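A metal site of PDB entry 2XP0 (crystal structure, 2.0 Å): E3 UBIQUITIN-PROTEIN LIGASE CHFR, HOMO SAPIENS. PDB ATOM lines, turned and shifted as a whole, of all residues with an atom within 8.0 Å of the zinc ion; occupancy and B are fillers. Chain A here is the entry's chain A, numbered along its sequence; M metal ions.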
ATOM      1  N   THR A  96       8.190 -16.244  10.281  1.00  0.00           N
ATOM      2  CA  THR A  96       8.373 -15.480  11.509  1.00  0.00           C
ATOM      3  C   THR A  96       9.365 -14.312  11.342  1.00  0.00           C
ATOM      4  O   THR A  96       9.295 -13.325  12.069  1.00  0.00           O
ATOM      5  CB  THR A  96       8.876 -16.442  12.614  1.00  0.00           C
ATOM      6  OG1 THR A  96       7.955 -17.537  12.738  1.00  0.00           O
ATOM      7  CG2 THR A  96       9.036 -15.716  13.934  1.00  0.00           C
ATOM      8  N   GLN A 119      10.715 -24.824   9.649  1.00  0.00           N
ATOM      9  CA  GLN A 119      10.593 -24.375  11.029  1.00  0.00           C
ATOM     10  C   GLN A 119      11.846 -24.641  11.840  1.00  0.00           C
ATOM     11  O   GLN A 119      12.621 -25.530  11.512  1.00  0.00           O
ATOM     12  CB  GLN A 119       9.390 -25.056  11.713  1.00  0.00           C
ATOM     13  CG  GLN A 119       9.591 -26.520  12.103  1.00  0.00           C
ATOM     14  CD  GLN A 119       8.376 -27.090  12.833  1.00  0.00           C
ATOM     15  OE1 GLN A 119       7.277 -26.565  12.740  1.00  0.00           O
ATOM     16  NE2 GLN A 119       8.593 -28.169  13.577  1.00  0.00           N
ATOM     17  N   CYS A 120      12.024 -23.862  12.901  1.00  0.00           N
ATOM     18  CA  CYS A 120      13.111 -24.041  13.860  1.00  0.00           C
ATOM     19  C   CYS A 120      12.822 -25.235  14.756  1.00  0.00           C
ATOM     20  O   CYS A 120      11.741 -25.322  15.342  1.00  0.00           O
ATOM     21  CB  CYS A 120      13.255 -22.770  14.722  1.00  0.00           C
ATOM     22  SG  CYS A 120      14.479 -22.877  16.041  1.00  0.00           S
ATOM     23  N   ALA A 121      13.773 -26.164  14.851  1.00  0.00           N
ATOM     24  CA  ALA A 121      13.558 -27.379  15.642  1.00  0.00           C
ATOM     25  C   ALA A 121      13.523 -27.110  17.147  1.00  0.00           C
ATOM     26  O   ALA A 121      13.147 -27.979  17.934  1.00  0.00           O
ATOM     27  CB  ALA A 121      14.615 -28.425  15.315  1.00  0.00           C
ATOM     28  N   VAL A 122      13.925 -25.901  17.538  1.00  0.00           N
ATOM     29  CA  VAL A 122      13.952 -25.526  18.947  1.00  0.00           C
ATOM     30  C   VAL A 122      12.653 -24.818  19.376  1.00  0.00           C
ATOM     31  O   VAL A 122      12.000 -25.241  20.326  1.00  0.00           O
ATOM     32  CB  VAL A 122      15.188 -24.653  19.273  1.00  0.00           C
ATOM     33  CG1 VAL A 122      15.153 -24.172  20.735  1.00  0.00           C
ATOM     34  CG2 VAL A 122      16.462 -25.435  18.996  1.00  0.00           C
ATOM     35  N   CYS A 123      12.275 -23.755  18.664  1.00  0.00           N
ATOM     36  CA  CYS A 123      11.096 -22.989  19.089  1.00  0.00           C
ATOM     37  C   CYS A 123       9.866 -23.347  18.272  1.00  0.00           C
ATOM     38  O   CYS A 123       8.772 -22.890  18.583  1.00  0.00           O
ATOM     39  CB  CYS A 123      11.375 -21.490  18.978  1.00  0.00           C
ATOM     40  SG  CYS A 123      11.565 -20.936  17.266  1.00  0.00           S
ATOM     41  N   LEU A 124      10.078 -24.130  17.211  1.00  0.00           N
ATOM     42  CA  LEU A 124       8.999 -24.664  16.382  1.00  0.00           C
ATOM     43  C   LEU A 124       8.234 -23.612  15.575  1.00  0.00           C
ATOM     44  O   LEU A 124       7.206 -23.918  14.981  1.00  0.00           O
ATOM     45  CB  LEU A 124       8.042 -25.536  17.201  1.00  0.00           C
ATOM     46  CG  LEU A 124       8.736 -26.636  18.018  1.00  0.00           C
ATOM     47  CD1 LEU A 124       7.737 -27.407  18.878  1.00  0.00           C
ATOM     48  CD2 LEU A 124       9.503 -27.587  17.103  1.00  0.00           C
ATOM     49  N   GLN A 125       8.741 -22.384  15.556  1.00  0.00           N
ATOM     50  CA  GLN A 125       8.136 -21.334  14.733  1.00  0.00           C
ATOM     51  C   GLN A 125       8.570 -21.470  13.265  1.00  0.00           C
ATOM     52  O   GLN A 125       9.663 -21.965  12.992  1.00  0.00           O
ATOM     53  CB  GLN A 125       8.471 -19.956  15.289  1.00  0.00           C
ATOM     54  CG  GLN A 125       7.939 -19.757  16.704  1.00  0.00           C
ATOM     55  CD  GLN A 125       6.504 -20.276  16.852  1.00  0.00           C
ATOM     56  OE1 GLN A 125       5.585 -19.764  16.219  1.00  0.00           O
ATOM     57  NE2 GLN A 125       6.318 -21.313  17.685  1.00  0.00           N
ATOM     58  N   PRO A 126       7.713 -21.035  12.321  1.00  0.00           N
ATOM     59  CA  PRO A 126       8.035 -21.190  10.895  1.00  0.00           C
ATOM     60  C   PRO A 126       9.001 -20.116  10.375  1.00  0.00           C
ATOM     61  O   PRO A 126       8.883 -18.953  10.751  1.00  0.00           O
ATOM     62  CB  PRO A 126       6.658 -21.035  10.218  1.00  0.00           C
ATOM     63  CG  PRO A 126       5.881 -20.174  11.140  1.00  0.00           C
ATOM     64  CD  PRO A 126       6.342 -20.535  12.543  1.00  0.00           C
ATOM     65  N   PHE A 127       9.924 -20.521   9.505  1.00  0.00           N
ATOM     66  CA  PHE A 127      10.817 -19.585   8.818  1.00  0.00           C
ATOM     67  C   PHE A 127      11.000 -20.067   7.393  1.00  0.00           C
ATOM     68  O   PHE A 127      11.023 -21.269   7.160  1.00  0.00           O
ATOM     69  CB  PHE A 127      12.193 -19.524   9.496  1.00  0.00           C
ATOM     70  CG  PHE A 127      12.171 -18.929  10.865  1.00  0.00           C
ATOM     71  CD1 PHE A 127      12.410 -17.570  11.041  1.00  0.00           C
ATOM     72  CD2 PHE A 127      11.924 -19.708  11.964  1.00  0.00           C
ATOM     73  CE1 PHE A 127      12.402 -17.009  12.309  1.00  0.00           C
ATOM     74  CE2 PHE A 127      11.896 -19.165  13.224  1.00  0.00           C
ATOM     75  CZ  PHE A 127      12.135 -17.807  13.400  1.00  0.00           C
ATOM     76  N   CYS A 142      17.856 -16.716   8.121  1.00  0.00           N
ATOM     77  CA  CYS A 142      17.190 -16.939   9.401  1.00  0.00           C
ATOM     78  C   CYS A 142      16.960 -18.396   9.833  1.00  0.00           C
ATOM     79  O   CYS A 142      16.460 -18.628  10.932  1.00  0.00           O
ATOM     80  CB  CYS A 142      15.856 -16.189   9.435  1.00  0.00           C
ATOM     81  SG  CYS A 142      14.787 -16.528   8.026  1.00  0.00           S
ATOM     82  N   LEU A 143      17.314 -19.351   8.989  1.00  0.00           N
ATOM     83  CA  LEU A 143      17.166 -20.764   9.344  1.00  0.00           C
ATOM     84  C   LEU A 143      18.331 -21.564   8.765  1.00  0.00           C
ATOM     85  O   LEU A 143      18.633 -21.432   7.586  1.00  0.00           O
ATOM     86  CB  LEU A 143      15.805 -21.322   8.852  1.00  0.00           C
ATOM     87  CG  LEU A 143      15.340 -22.686   9.389  1.00  0.00           C
ATOM     88  CD1 LEU A 143      15.045 -22.593  10.888  1.00  0.00           C
ATOM     89  CD2 LEU A 143      14.129 -23.251   8.629  1.00  0.00           C
ATOM     90  N   ASP A 201      19.164 -25.408  26.121  1.00  0.00           N
ATOM     91  CA  ASP A 201      18.442 -26.199  25.144  1.00  0.00           C
ATOM     92  C   ASP A 201      19.315 -27.425  24.931  1.00  0.00           C
ATOM     93  O   ASP A 201      20.110 -27.477  23.985  1.00  0.00           O
ATOM     94  CB  ASP A 201      18.257 -25.418  23.836  1.00  0.00           C
ATOM     95  CG  ASP A 201      17.336 -24.201  23.989  1.00  0.00           C
ATOM     96  OD1 ASP A 201      16.367 -24.273  24.781  1.00  0.00           O
ATOM     97  OD2 ASP A 201      17.567 -23.169  23.329  1.00  0.00           O
ATOM     98  N   VAL A 209      18.777 -27.867  13.061  1.00  0.00           N
ATOM     99  CA  VAL A 209      18.284 -26.774  12.216  1.00  0.00           C
ATOM    100  C   VAL A 209      17.479 -25.796  13.065  1.00  0.00           C
ATOM    101  O   VAL A 209      16.373 -26.109  13.515  1.00  0.00           O
ATOM    102  CB  VAL A 209      17.427 -27.300  11.062  1.00  0.00           C
ATOM    103  CG1 VAL A 209      16.729 -26.139  10.335  1.00  0.00           C
ATOM    104  CG2 VAL A 209      18.305 -28.089  10.098  1.00  0.00           C
ATOM    105  N   LEU A 210      18.038 -24.605  13.271  1.00  0.00           N
ATOM    106  CA  LEU A 210      17.392 -23.648  14.149  1.00  0.00           C
ATOM    107  C   LEU A 210      17.417 -22.232  13.596  1.00  0.00           C
ATOM    108  O   LEU A 210      18.073 -21.961  12.595  1.00  0.00           O
ATOM    109  CB  LEU A 210      17.971 -23.721  15.567  1.00  0.00           C
ATOM    110  CG  LEU A 210      19.486 -23.850  15.740  1.00  0.00           C
ATOM    111  CD1 LEU A 210      20.199 -22.716  15.008  1.00  0.00           C
ATOM    112  CD2 LEU A 210      19.883 -23.888  17.220  1.00  0.00           C
ATOM    113  N   CYS A 211      16.690 -21.323  14.247  1.00  0.00           N
ATOM    114  CA  CYS A 211      16.563 -19.971  13.737  1.00  0.00           C
ATOM    115  C   CYS A 211      17.619 -19.051  14.336  1.00  0.00           C
ATOM    116  O   CYS A 211      18.358 -19.418  15.238  1.00  0.00           O
ATOM    117  CB  CYS A 211      15.169 -19.398  14.043  1.00  0.00           C
ATOM    118  SG  CYS A 211      14.843 -19.037  15.813  1.00  0.00           S
ATOM    119  N   TYR A 212      17.664 -17.835  13.798  1.00  0.00           N
ATOM    120  CA  TYR A 212      18.604 -16.822  14.268  1.00  0.00           C
ATOM    121  C   TYR A 212      18.558 -16.619  15.777  1.00  0.00           C
ATOM    122  O   TYR A 212      19.585 -16.703  16.449  1.00  0.00           O
ATOM    123  CB  TYR A 212      18.314 -15.483  13.575  1.00  0.00           C
ATOM    124  CG  TYR A 212      19.078 -14.346  14.209  1.00  0.00           C
ATOM    125  CD1 TYR A 212      20.445 -14.211  14.020  1.00  0.00           C
ATOM    126  CD2 TYR A 212      18.425 -13.412  15.013  1.00  0.00           C
ATOM    127  CE1 TYR A 212      21.150 -13.162  14.605  1.00  0.00           C
ATOM    128  CE2 TYR A 212      19.110 -12.372  15.593  1.00  0.00           C
ATOM    129  CZ  TYR A 212      20.468 -12.256  15.396  1.00  0.00           C
ATOM    130  OH  TYR A 212      21.143 -11.211  15.989  1.00  0.00           O
ATOM    131  N   CYS A 213      17.367 -16.352  16.311  1.00  0.00           N
ATOM    132  CA  CYS A 213      17.214 -16.101  17.749  1.00  0.00           C
ATOM    133  C   CYS A 213      17.596 -17.294  18.646  1.00  0.00           C
ATOM    134  O   CYS A 213      18.269 -17.124  19.659  1.00  0.00           O
ATOM    135  CB  CYS A 213      15.810 -15.591  18.050  1.00  0.00           C
ATOM    136  SG  CYS A 213      15.450 -13.941  17.331  1.00  0.00           S
ATOM    137  N   CYS A 214      17.173 -18.500  18.299  1.00  0.00           N
ATOM    138  CA  CYS A 214      17.549 -19.679  19.083  1.00  0.00           C
ATOM    139  C   CYS A 214      19.055 -19.995  18.973  1.00  0.00           C
ATOM    140  O   CYS A 214      19.711 -20.356  19.962  1.00  0.00           O
ATOM    141  CB  CYS A 214      16.727 -20.899  18.672  1.00  0.00           C
ATOM    142  SG  CYS A 214      14.980 -20.790  19.121  1.00  0.00           S
ATOM    143  N   GLY A 215      19.608 -19.869  17.768  1.00  0.00           N
ATOM    144  CA  GLY A 215      21.036 -20.046  17.604  1.00  0.00           C
ATOM    145  C   GLY A 215      21.813 -19.012  18.413  1.00  0.00           C
ATOM    146  O   GLY A 215      22.832 -19.327  19.044  1.00  0.00           O
ATOM    147  N   ARG A 217      20.889 -17.407  21.127  1.00  0.00           N
ATOM    148  CA  ARG A 217      20.748 -17.728  22.537  1.00  0.00           C
ATOM    149  C   ARG A 217      21.758 -18.808  22.950  1.00  0.00           C
ATOM    150  O   ARG A 217      22.390 -18.703  23.989  1.00  0.00           O
ATOM    151  CB  ARG A 217      19.308 -18.165  22.826  1.00  0.00           C
ATOM    152  CG  ARG A 217      18.996 -18.424  24.288  1.00  0.00           C
ATOM    153  CD  ARG A 217      17.498 -18.688  24.495  1.00  0.00           C
ATOM    154  NE  ARG A 217      17.056 -19.907  23.839  1.00  0.00           N
ATOM    155  CZ  ARG A 217      16.234 -19.946  22.788  1.00  0.00           C
ATOM    156  NH1 ARG A 217      15.758 -18.818  22.283  1.00  0.00           N
ATOM    157  NH2 ARG A 217      15.868 -21.117  22.252  1.00  0.00           N
HETATM  158 ZN    ZN M   1      13.946 -20.860  17.002  1.00  0.00          ZN
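SG of Cys 120 is bound to the zinc ion (2.3 Å).
The zinc ion is bound by SG of Cys 211, at 2.4 Å.
The zinc ion is bound by SG of Cys 214 (2.4 Å).
The zinc ion is bound by SG of Cys 123 (2.4 Å).
The zinc ion has four donor atoms within binding distance.
The backbone carbonyl oxygen (O) of Gln 125 is in hydrogen-bond range of the backbone NH (N) of Cys 120, 3.0 Å away.
The side-chain sulfur (SG) of Cys 120 lies close to the backbone NH (N) of Val 122, 3.4 Å away.
NH2 of Arg 217 lies close to SG of Cys 214, at 3.3 Å.
The side-chain sulfur (SG) of Cys 211 sits close to the backbone NH (N) of Cys 213 (3.7 Å).
O of Cys 123 is in hydrogen-bond range of NE2 of Gln 125, 3.1 Å away.
Four residues have an atom within 4 Å of the zinc ion: Cys 120, Cys 123, Cys 211 and Cys 214.
The nearest printed residue that does not touch the zinc ion is Val 122 (4.6 Å).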
